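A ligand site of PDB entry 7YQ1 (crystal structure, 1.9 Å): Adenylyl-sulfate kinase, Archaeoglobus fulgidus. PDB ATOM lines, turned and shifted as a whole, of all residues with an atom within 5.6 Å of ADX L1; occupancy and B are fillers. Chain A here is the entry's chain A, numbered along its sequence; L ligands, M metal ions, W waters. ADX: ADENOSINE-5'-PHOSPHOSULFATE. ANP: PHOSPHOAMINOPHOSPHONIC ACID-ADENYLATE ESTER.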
ATOM      1  N   PRO A  13     -12.386  28.816   8.271  1.00  0.00           N
ATOM      2  CA  PRO A  13     -12.683  27.404   8.548  1.00  0.00           C
ATOM      3  C   PRO A  13     -11.457  26.546   8.316  1.00  0.00           C
ATOM      4  O   PRO A  13     -10.417  26.992   7.828  1.00  0.00           O
ATOM      5  CB  PRO A  13     -13.804  27.076   7.558  1.00  0.00           C
ATOM      6  CG  PRO A  13     -13.588  28.020   6.430  1.00  0.00           C
ATOM      7  CD  PRO A  13     -13.044  29.292   7.033  1.00  0.00           C
ATOM      8  N   SER A  14     -11.596  25.271   8.679  1.00  0.00           N
ATOM      9  CA  SER A  14     -10.460  24.352   8.590  1.00  0.00           C
ATOM     10  C   SER A  14     -10.044  24.160   7.144  1.00  0.00           C
ATOM     11  O   SER A  14     -10.872  23.958   6.258  1.00  0.00           O
ATOM     12  CB  SER A  14     -10.831  23.010   9.214  1.00  0.00           C
ATOM     13  OG  SER A  14      -9.791  22.075   9.019  1.00  0.00           O
ATOM     14  N   GLY A  15      -8.730  24.235   6.903  1.00  0.00           N
ATOM     15  CA  GLY A  15      -8.196  24.080   5.556  1.00  0.00           C
ATOM     16  C   GLY A  15      -8.213  25.334   4.716  1.00  0.00           C
ATOM     17  O   GLY A  15      -7.857  25.271   3.535  1.00  0.00           O
ATOM     18  N   LYS A  18      -4.913  29.253   6.920  1.00  0.00           N
ATOM     19  CA  LYS A  18      -4.567  30.248   7.936  1.00  0.00           C
ATOM     20  C   LYS A  18      -3.111  30.101   8.390  1.00  0.00           C
ATOM     21  O   LYS A  18      -2.351  31.077   8.419  1.00  0.00           O
ATOM     22  CB  LYS A  18      -5.502  30.123   9.142  1.00  0.00           C
ATOM     23  CG  LYS A  18      -6.979  30.260   8.840  1.00  0.00           C
ATOM     24  CD  LYS A  18      -7.834  30.058  10.094  1.00  0.00           C
ATOM     25  CE  LYS A  18      -7.593  28.709  10.769  1.00  0.00           C
ATOM     26  NZ  LYS A  18      -8.303  27.586  10.084  1.00  0.00           N
ATOM     27  N   GLY A  41      -3.840  28.396  16.613  1.00  0.00           N
ATOM     28  CA  GLY A  41      -4.839  27.742  17.441  1.00  0.00           C
ATOM     29  C   GLY A  41      -4.436  26.338  17.854  1.00  0.00           C
ATOM     30  O   GLY A  41      -4.534  25.965  19.027  1.00  0.00           O
ATOM     31  N   ASP A  42      -3.947  25.556  16.902  1.00  0.00           N
ATOM     32  CA  ASP A  42      -3.548  24.191  17.212  1.00  0.00           C
ATOM     33  C   ASP A  42      -2.316  24.170  18.110  1.00  0.00           C
ATOM     34  O   ASP A  42      -2.226  23.342  19.034  1.00  0.00           O
ATOM     35  CB  ASP A  42      -3.282  23.420  15.924  1.00  0.00           C
ATOM     36  CG  ASP A  42      -3.491  21.938  16.094  1.00  0.00           C
ATOM     37  OD1 ASP A  42      -3.626  21.504  17.242  1.00  0.00           O
ATOM     38  OD2 ASP A  42      -3.582  21.224  15.066  1.00  0.00           O
ATOM     39  N   ARG A  45      -3.323  25.256  21.721  1.00  0.00           N
ATOM     40  CA  ARG A  45      -4.117  24.210  22.357  1.00  0.00           C
ATOM     41  C   ARG A  45      -3.229  23.078  22.879  1.00  0.00           C
ATOM     42  O   ARG A  45      -3.352  22.668  24.042  1.00  0.00           O
ATOM     43  CB  ARG A  45      -5.146  23.663  21.379  1.00  0.00           C
ATOM     44  CG  ARG A  45      -6.472  24.429  21.332  1.00  0.00           C
ATOM     45  CD  ARG A  45      -7.324  23.930  20.171  1.00  0.00           C
ATOM     46  NE  ARG A  45      -8.631  24.573  20.119  1.00  0.00           N
ATOM     47  CZ  ARG A  45      -9.699  24.152  20.796  1.00  0.00           C
ATOM     48  NH1 ARG A  45      -9.624  23.109  21.617  1.00  0.00           N
ATOM     49  NH2 ARG A  45     -10.859  24.786  20.644  1.00  0.00           N
ATOM     50  N   PHE A  54     -14.163  21.021  21.568  1.00  0.00           N
ATOM     51  CA  PHE A  54     -14.572  21.992  20.563  1.00  0.00           C
ATOM     52  C   PHE A  54     -16.032  22.398  20.682  1.00  0.00           C
ATOM     53  O   PHE A  54     -16.624  22.826  19.687  1.00  0.00           O
ATOM     54  CB  PHE A  54     -14.278  21.444  19.163  1.00  0.00           C
ATOM     55  CG  PHE A  54     -12.817  21.369  18.839  1.00  0.00           C
ATOM     56  CD1 PHE A  54     -12.075  20.249  19.197  1.00  0.00           C
ATOM     57  CD2 PHE A  54     -12.178  22.429  18.216  1.00  0.00           C
ATOM     58  CE1 PHE A  54     -10.721  20.179  18.910  1.00  0.00           C
ATOM     59  CE2 PHE A  54     -10.821  22.372  17.932  1.00  0.00           C
ATOM     60  CZ  PHE A  54     -10.092  21.248  18.286  1.00  0.00           C
ATOM     61  N   ARG A  59     -14.186  26.490  22.902  1.00  0.00           N
ATOM     62  CA  ARG A  59     -13.510  27.339  21.926  1.00  0.00           C
ATOM     63  C   ARG A  59     -13.475  28.779  22.398  1.00  0.00           C
ATOM     64  O   ARG A  59     -12.475  29.487  22.195  1.00  0.00           O
ATOM     65  CB  ARG A  59     -14.202  27.264  20.566  1.00  0.00           C
ATOM     66  CG  ARG A  59     -14.297  25.894  19.926  1.00  0.00           C
ATOM     67  CD  ARG A  59     -15.162  26.003  18.676  1.00  0.00           C
ATOM     68  NE  ARG A  59     -15.413  24.734  18.007  1.00  0.00           N
ATOM     69  CZ  ARG A  59     -15.122  24.497  16.729  1.00  0.00           C
ATOM     70  NH1 ARG A  59     -14.415  25.356  16.023  1.00  0.00           N
ATOM     71  NH2 ARG A  59     -15.559  23.379  16.163  1.00  0.00           N
ATOM     72  N   HIS A  62     -10.708  29.396  24.822  1.00  0.00           N
ATOM     73  CA  HIS A  62      -9.424  29.378  24.131  1.00  0.00           C
ATOM     74  C   HIS A  62      -9.221  30.667  23.346  1.00  0.00           C
ATOM     75  O   HIS A  62      -8.124  31.259  23.367  1.00  0.00           O
ATOM     76  CB  HIS A  62      -9.370  28.133  23.243  1.00  0.00           C
ATOM     77  CG  HIS A  62      -8.341  28.180  22.159  1.00  0.00           C
ATOM     78  ND1 HIS A  62      -7.004  28.353  22.405  1.00  0.00           N
ATOM     79  CD2 HIS A  62      -8.464  28.010  20.816  1.00  0.00           C
ATOM     80  CE1 HIS A  62      -6.338  28.318  21.267  1.00  0.00           C
ATOM     81  NE2 HIS A  62      -7.200  28.114  20.284  1.00  0.00           N
ATOM     82  N   ASN A  63     -10.273  31.156  22.698  1.00  0.00           N
ATOM     83  CA  ASN A  63     -10.175  32.435  21.997  1.00  0.00           C
ATOM     84  C   ASN A  63      -9.879  33.587  22.948  1.00  0.00           C
ATOM     85  O   ASN A  63      -9.069  34.459  22.635  1.00  0.00           O
ATOM     86  CB  ASN A  63     -11.453  32.700  21.198  1.00  0.00           C
ATOM     87  CG  ASN A  63     -11.424  32.094  19.798  1.00  0.00           C
ATOM     88  OD1 ASN A  63     -11.382  32.809  18.806  1.00  0.00           O
ATOM     89  ND2 ASN A  63     -11.445  30.758  19.725  1.00  0.00           N
ATOM     90  N   SER A  83      -3.517  32.821  14.206  1.00  0.00           N
ATOM     91  CA  SER A  83      -4.097  31.932  13.201  1.00  0.00           C
ATOM     92  C   SER A  83      -4.997  30.936  13.922  1.00  0.00           C
ATOM     93  O   SER A  83      -4.591  29.837  14.296  1.00  0.00           O
ATOM     94  CB  SER A  83      -3.014  31.241  12.360  1.00  0.00           C
ATOM     95  OG  SER A  83      -2.107  30.513  13.156  1.00  0.00           O
ATOM     96  N   VAL A  84      -6.267  31.341  14.115  1.00  0.00           N
ATOM     97  CA  VAL A  84      -7.230  30.523  14.835  1.00  0.00           C
ATOM     98  C   VAL A  84      -8.568  30.579  14.098  1.00  0.00           C
ATOM     99  O   VAL A  84      -8.920  31.595  13.485  1.00  0.00           O
ATOM    100  CB  VAL A  84      -7.414  30.975  16.306  1.00  0.00           C
ATOM    101  CG1 VAL A  84      -6.078  30.969  17.053  1.00  0.00           C
ATOM    102  CG2 VAL A  84      -8.072  32.336  16.394  1.00  0.00           C
ATOM    103  N   VAL A  85      -9.309  29.478  14.175  1.00  0.00           N
ATOM    104  CA  VAL A  85     -10.576  29.364  13.451  1.00  0.00           C
ATOM    105  C   VAL A  85     -11.480  30.559  13.766  1.00  0.00           C
ATOM    106  O   VAL A  85     -11.950  31.260  12.852  1.00  0.00           O
ATOM    107  CB  VAL A  85     -11.267  28.027  13.777  1.00  0.00           C
ATOM    108  CG1 VAL A  85     -12.639  27.963  13.138  1.00  0.00           C
ATOM    109  CG2 VAL A  85     -10.398  26.866  13.299  1.00  0.00           C
ATOM    110  N   SER A  86     -11.678  30.841  15.057  1.00  0.00           N
ATOM    111  CA  SER A  86     -12.489  31.942  15.569  1.00  0.00           C
ATOM    112  C   SER A  86     -13.794  32.039  14.797  1.00  0.00           C
ATOM    113  O   SER A  86     -14.012  33.001  14.044  1.00  0.00           O
ATOM    114  CB  SER A  86     -11.720  33.276  15.525  1.00  0.00           C
ATOM    115  OG  SER A  86     -11.094  33.487  14.272  1.00  0.00           O
ATOM    116  N   PRO A  87     -14.692  31.066  14.956  1.00  0.00           N
ATOM    117  CA  PRO A  87     -15.803  30.904  14.007  1.00  0.00           C
ATOM    118  C   PRO A  87     -16.962  31.895  14.149  1.00  0.00           C
ATOM    119  O   PRO A  87     -17.816  31.919  13.253  1.00  0.00           O
ATOM    120  CB  PRO A  87     -16.283  29.466  14.274  1.00  0.00           C
ATOM    121  CG  PRO A  87     -15.850  29.156  15.669  1.00  0.00           C
ATOM    122  CD  PRO A  87     -14.592  29.948  15.914  1.00  0.00           C
ATOM    123  N   TRP A  91     -16.999  36.849  18.748  1.00  0.00           N
ATOM    124  CA  TRP A  91     -15.680  36.673  19.345  1.00  0.00           C
ATOM    125  C   TRP A  91     -14.649  37.531  18.643  1.00  0.00           C
ATOM    126  O   TRP A  91     -13.739  38.074  19.288  1.00  0.00           O
ATOM    127  CB  TRP A  91     -15.270  35.201  19.275  1.00  0.00           C
ATOM    128  CG  TRP A  91     -16.242  34.278  19.924  1.00  0.00           C
ATOM    129  CD1 TRP A  91     -17.356  34.606  20.646  1.00  0.00           C
ATOM    130  CD2 TRP A  91     -16.198  32.849  19.891  1.00  0.00           C
ATOM    131  NE1 TRP A  91     -18.005  33.481  21.065  1.00  0.00           N
ATOM    132  CE2 TRP A  91     -17.317  32.379  20.615  1.00  0.00           C
ATOM    133  CE3 TRP A  91     -15.322  31.914  19.333  1.00  0.00           C
ATOM    134  CZ2 TRP A  91     -17.579  31.027  20.794  1.00  0.00           C
ATOM    135  CZ3 TRP A  91     -15.590  30.564  19.504  1.00  0.00           C
ATOM    136  CH2 TRP A  91     -16.707  30.138  20.233  1.00  0.00           C
ATOM    137  N   LYS A 120      -3.976  16.932   7.105  1.00  0.00           N
ATOM    138  CA  LYS A 120      -4.233  16.323   8.398  1.00  0.00           C
ATOM    139  C   LYS A 120      -5.415  15.360   8.370  1.00  0.00           C
ATOM    140  O   LYS A 120      -5.594  14.594   9.328  1.00  0.00           O
ATOM    141  CB  LYS A 120      -4.492  17.400   9.463  1.00  0.00           C
ATOM    142  CG  LYS A 120      -3.315  18.324   9.728  1.00  0.00           C
ATOM    143  CD  LYS A 120      -3.651  19.295  10.850  1.00  0.00           C
ATOM    144  CE  LYS A 120      -4.268  20.582  10.296  1.00  0.00           C
ATOM    145  NZ  LYS A 120      -4.187  21.707  11.264  1.00  0.00           N
ATOM    146  N   LEU A 122      -8.778  15.997   8.397  1.00  0.00           N
ATOM    147  CA  LEU A 122      -9.882  16.307   9.297  1.00  0.00           C
ATOM    148  C   LEU A 122     -11.227  16.125   8.607  1.00  0.00           C
ATOM    149  O   LEU A 122     -12.183  15.644   9.229  1.00  0.00           O
ATOM    150  CB  LEU A 122      -9.741  17.737   9.829  1.00  0.00           C
ATOM    151  CG  LEU A 122      -8.530  17.999  10.726  1.00  0.00           C
ATOM    152  CD1 LEU A 122      -8.355  19.486  10.992  1.00  0.00           C
ATOM    153  CD2 LEU A 122      -8.671  17.235  12.029  1.00  0.00           C
ATOM    154  N   ILE A 131     -15.179  12.609  13.905  1.00  0.00           N
ATOM    155  CA  ILE A 131     -15.294  13.835  14.696  1.00  0.00           C
ATOM    156  C   ILE A 131     -16.555  14.549  14.248  1.00  0.00           C
ATOM    157  O   ILE A 131     -17.011  14.406  13.104  1.00  0.00           O
ATOM    158  CB  ILE A 131     -14.060  14.749  14.573  1.00  0.00           C
ATOM    159  CG1 ILE A 131     -13.976  15.378  13.184  1.00  0.00           C
ATOM    160  CG2 ILE A 131     -12.782  13.995  14.918  1.00  0.00           C
ATOM    161  CD1 ILE A 131     -12.594  15.910  12.825  1.00  0.00           C
ATOM    162  N   LYS A 132     -17.130  15.341  15.153  1.00  0.00           N
ATOM    163  CA  LYS A 132     -18.387  16.030  14.886  1.00  0.00           C
ATOM    164  C   LYS A 132     -18.167  17.530  14.952  1.00  0.00           C
ATOM    165  O   LYS A 132     -17.384  18.016  15.774  1.00  0.00           O
ATOM    166  CB  LYS A 132     -19.471  15.595  15.875  1.00  0.00           C
ATOM    167  CG  LYS A 132     -20.094  14.241  15.551  1.00  0.00           C
ATOM    168  CD  LYS A 132     -21.405  14.395  14.796  1.00  0.00           C
ATOM    169  CE  LYS A 132     -22.136  13.068  14.687  1.00  0.00           C
ATOM    170  NZ  LYS A 132     -23.517  13.141  15.263  1.00  0.00           N
ATOM    171  N   GLY A 133     -18.863  18.256  14.088  1.00  0.00           N
ATOM    172  CA  GLY A 133     -18.806  19.697  14.111  1.00  0.00           C
ATOM    173  C   GLY A 133     -17.495  20.290  13.646  1.00  0.00           C
ATOM    174  O   GLY A 133     -17.043  21.291  14.213  1.00  0.00           O
ATOM    175  N   LEU A 134     -16.872  19.702  12.630  1.00  0.00           N
ATOM    176  CA  LEU A 134     -15.686  20.310  12.027  1.00  0.00           C
ATOM    177  C   LEU A 134     -16.060  21.626  11.380  1.00  0.00           C
ATOM    178  O   LEU A 134     -16.921  21.674  10.487  1.00  0.00           O
ATOM    179  CB  LEU A 134     -15.070  19.358  10.998  1.00  0.00           C
ATOM    180  CG  LEU A 134     -13.794  19.859  10.310  1.00  0.00           C
ATOM    181  CD1 LEU A 134     -12.608  19.899  11.289  1.00  0.00           C
ATOM    182  CD2 LEU A 134     -13.460  19.041   9.081  1.00  0.00           C
ATOM    183  N   THR A 135     -15.423  22.717  11.819  1.00  0.00           N
ATOM    184  CA  THR A 135     -15.686  24.020  11.238  1.00  0.00           C
ATOM    185  C   THR A 135     -15.270  24.040   9.767  1.00  0.00           C
ATOM    186  O   THR A 135     -14.092  23.867   9.441  1.00  0.00           O
ATOM    187  CB  THR A 135     -14.942  25.122  11.996  1.00  0.00           C
ATOM    188  OG1 THR A 135     -15.176  24.970  13.404  1.00  0.00           O
ATOM    189  CG2 THR A 135     -15.437  26.479  11.526  1.00  0.00           C
HETATM  190  SB  ADX L   1     -11.245  27.465  17.602  1.00  0.00           S
HETATM  191  O1B ADX L   1     -11.054  26.952  19.064  1.00  0.00           O
HETATM  192  O2B ADX L   1     -12.680  27.497  17.215  1.00  0.00           O
HETATM  193  O3B ADX L   1     -10.832  28.920  17.401  1.00  0.00           O
HETATM  194  PA  ADX L   1      -8.759  26.349  16.640  1.00  0.00           P
HETATM  195  O1A ADX L   1      -8.245  26.452  18.108  1.00  0.00           O
HETATM  196  O2A ADX L   1      -8.094  27.358  15.791  1.00  0.00           O
HETATM  197  O3A ADX L   1     -10.416  26.507  16.543  1.00  0.00           O
HETATM  198  O5' ADX L   1      -8.555  24.820  16.020  1.00  0.00           O
HETATM  199  C5' ADX L   1      -7.405  24.032  16.164  1.00  0.00           C
HETATM  200  C4' ADX L   1      -7.486  22.882  15.129  1.00  0.00           C
HETATM  201  O4' ADX L   1      -8.754  21.984  15.399  1.00  0.00           O
HETATM  202  C3' ADX L   1      -7.631  23.311  13.965  1.00  0.00           C
HETATM  203  O3' ADX L   1      -6.932  22.419  13.005  1.00  0.00           O
HETATM  204  C2' ADX L   1      -9.255  23.162  13.638  1.00  0.00           C
HETATM  205  O2' ADX L   1      -9.544  23.295  12.232  1.00  0.00           O
HETATM  206  C1' ADX L   1      -9.520  22.007  14.066  1.00  0.00           C
HETATM  207  N9  ADX L   1     -11.039  21.981  14.238  1.00  0.00           N
HETATM  208  C8  ADX L   1     -12.054  22.795  13.937  1.00  0.00           C
HETATM  209  N7  ADX L   1     -13.203  22.212  14.354  1.00  0.00           N
HETATM  210  C5  ADX L   1     -12.879  21.040  14.903  1.00  0.00           C
HETATM  211  C6  ADX L   1     -13.668  20.066  15.471  1.00  0.00           C
HETATM  212  N6  ADX L   1     -15.115  19.906  15.713  1.00  0.00           N
HETATM  213  N1  ADX L   1     -13.120  18.959  15.972  1.00  0.00           N
HETATM  214  C2  ADX L   1     -11.789  18.790  15.908  1.00  0.00           C
HETATM  215  N3  ADX L   1     -10.982  19.771  15.329  1.00  0.00           N
HETATM  216  C4  ADX L   1     -11.541  20.877  14.836  1.00  0.00           C
HETATM  217  PG  ANP L   2      -6.715  24.324  10.369  1.00  0.00           P
HETATM  218  O1G ANP L   2      -5.536  24.663  11.231  1.00  0.00           O
HETATM  219  O2G ANP L   2      -7.057  22.867  10.524  1.00  0.00           O
HETATM  220  O3G ANP L   2      -7.895  25.189  10.747  1.00  0.00           O
HETATM  221  PB  ANP L   2      -5.618  26.070   8.179  1.00  0.00           P
HETATM  222  O1B ANP L   2      -6.691  27.094   7.971  1.00  0.00           O
HETATM  223  O2B ANP L   2      -4.577  26.570   9.180  1.00  0.00           O
HETATM  224  N3B ANP L   2      -6.293  24.589   8.674  1.00  0.00           N
HETATM  225  PA  ANP L   2      -3.395  25.396   6.396  1.00  0.00           P
HETATM  226  O1A ANP L   2      -2.539  26.623   6.575  1.00  0.00           O
HETATM  227  O2A ANP L   2      -2.933  24.216   7.256  1.00  0.00           O
HETATM  228  O3A ANP L   2      -4.967  25.783   6.712  1.00  0.00           O
HETATM  229  O5' ANP L   2      -3.427  24.968   4.798  1.00  0.00           O
HETATM  230  C5' ANP L   2      -4.048  23.728   4.471  1.00  0.00           C
HETATM  231  C4' ANP L   2      -3.407  23.192   3.214  1.00  0.00           C
HETATM  232  O4' ANP L   2      -3.718  24.230   2.019  1.00  0.00           O
HETATM  233  C3' ANP L   2      -2.093  23.118   3.321  1.00  0.00           C
HETATM  234  O3' ANP L   2      -1.629  21.930   2.587  1.00  0.00           O
HETATM  235  C2' ANP L   2      -1.532  24.366   2.602  1.00  0.00           C
HETATM  236  O2' ANP L   2      -0.287  24.098   2.119  1.00  0.00           O
HETATM  237  C1' ANP L   2      -2.565  24.493   1.461  1.00  0.00           C
HETATM  238  N9  ANP L   2      -2.613  25.788   0.807  1.00  0.00           N
HETATM  239  C8  ANP L   2      -2.558  26.716   1.800  1.00  0.00           C
HETATM  240  N7  ANP L   2      -2.611  27.897   1.179  1.00  0.00           N
HETATM  241  C5  ANP L   2      -2.700  27.681  -0.157  1.00  0.00           C
HETATM  242  C6  ANP L   2      -2.785  28.533  -1.242  1.00  0.00           C
HETATM  243  N6  ANP L   2      -2.814  29.979  -1.478  1.00  0.00           N
HETATM  244  N1  ANP L   2      -2.860  28.047  -2.440  1.00  0.00           N
HETATM  245  C2  ANP L   2      -2.857  26.695  -2.652  1.00  0.00           C
HETATM  246  N3  ANP L   2      -2.774  25.851  -1.591  1.00  0.00           N
HETATM  247  C4  ANP L   2      -2.698  26.359  -0.369  1.00  0.00           C
HETATM  248 MG    MG M   1      -3.921  25.741  10.921  1.00  0.00          MG
HETATM  249  O   HOH W   1      -6.370  21.232  17.943  1.00  0.00           O
HETATM  250  O   HOH W   2      -5.768  26.767  14.392  1.00  0.00           O
HETATM  251  O   HOH W   3     -14.695  16.909  17.627  1.00  0.00           O
HETATM  252  O   HOH W   4      -6.167  20.192  13.907  1.00  0.00           O
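The guanidinium group of Arg 45 is in salt-bridge range of an oxygen (O1B) of ADX L1. N6 of ADX L1 sits at hydrogen-bond distance from O of Gly 133 (2.8 Å). O2A of ADX L1 lies within hydrogen-bond range of N of Val 85. A ring nitrogen (NE2) of His 62 lies within hydrogen-bond range of an oxygen (O1A) of ADX L1. A nitrogen (N6) of ADX L1 lies within hydrogen-bond range of the backbone carbonyl oxygen (O) of Lys 132 (3.0 Å). The guanidinium group of Arg 59 lies within salt-bridge range of an oxygen (O2B) of ADX L1 (3.0 Å). O3B of ADX L1 is in hydrogen-bond range of ND2 of Asn 63 (3.0 Å). An oxygen (O3B) of ADX L1 sits at hydrogen-bond distance from the backbone NH (N) of Ser 86, 3.1 Å away. An oxygen (O2') of ADX L1 sits close to the side-chain hydroxyl (OG) of Ser 14. The side-chain amino group (NZ) of Lys 120 is in hydrogen-bond range of an oxygen (O3') of ADX L1 (3.3 Å). The backbone NH (N) of Thr 135 sits at hydrogen-bond distance from a nitrogen (N7) of ADX L1. The side-chain hydroxyl of Ser 14 lies within hydrogen-bond range of an oxygen (O2G) of ANP L2 (3.2 Å). The side-chain amino group of Lys 120 is in salt-bridge range of an oxygen (O2G) of ANP L2. O1B of ANP L2 lies within hydrogen-bond range of N of Lys 18, at 3.0 Å. The side-chain amino group of Lys 18 lies within salt-bridge range of an oxygen (O3G) of ANP L2 (2.5 Å).
An oxygen (O3') of ADX L1 is in hydrogen-bond range of an oxygen (O2G) of ANP L2, 2.5 Å away.
NH2 of Arg 59 is in hydrogen-bond range of O of Gly 133 (3.2 Å). ND2 of Asn 63 lies within hydrogen-bond range of O of Arg 59, 3.0 Å away. O of Phe 54 lies within hydrogen-bond range of NE of Arg 59 (2.8 Å). The guanidinium group (NH1) of Arg 59 lies within hydrogen-bond range of the side-chain hydroxyl (OG1) of Thr 135 (2.8 Å). The side-chain hydroxyl of Ser 86 is in hydrogen-bond range of the backbone carbonyl oxygen of Val 84 (3.0 Å). O of Thr 135 sits at hydrogen-bond distance from N of Ser 14 (3.0 Å). NZ of Lys 120 is in salt-bridge range of OD2 of Asp 42 (3.9 Å). The backbone NH of Gly 41 is in hydrogen-bond range of the backbone carbonyl oxygen of Ser 83.
Merely in contact with ADX L1: Gly 41 (3.7 Å), Asp 42 (3.9 Å), Phe 54 (3.3 Å), Val 84 (3.4 Å), Pro 87 (3.4 Å), Leu 122 (3.8 Å) and Leu 134 (3.6 Å). Hydrophobic or aromatic side chains within 4 Å of ADX L1: Phe 54, His 62, Val 84, Val 85, Pro 87, Leu 122 and Leu 134. 18 residues have an atom within 4 Å of ADX L1: Ser 14, Gly 41, Asp 42, Arg 45, Phe 54, Arg 59, His 62, Asn 63, Val 84, Val 85, Ser 86, Pro 87, Lys 120, Leu 122, Lys 132, Gly 133, Leu 134 and Thr 135. Along chain A the residues within 4 Å of ADX L1 span positions 14 to 135. The nearest printed residue that does not touch ADX L1 is Ile 131 (4.3 Å).
Water W4 bridges an oxygen (O3') of ADX L1 (2.5 Å) and the side-chain carboxylate (OD2) of Asp 42 (3.0 Å). Water W2 lies within hydrogen-bond range of O2A of ADX L1 (2.8 Å), O of Ser 83 (3.3 Å), N of Asp 42 (3.3 Å) and N of Gly 41 (3.4 Å). Water W3 bridges a nitrogen (N1) of ADX L1 (3.1 Å) and the backbone carbonyl oxygen of Lys 132 (3.4 Å).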
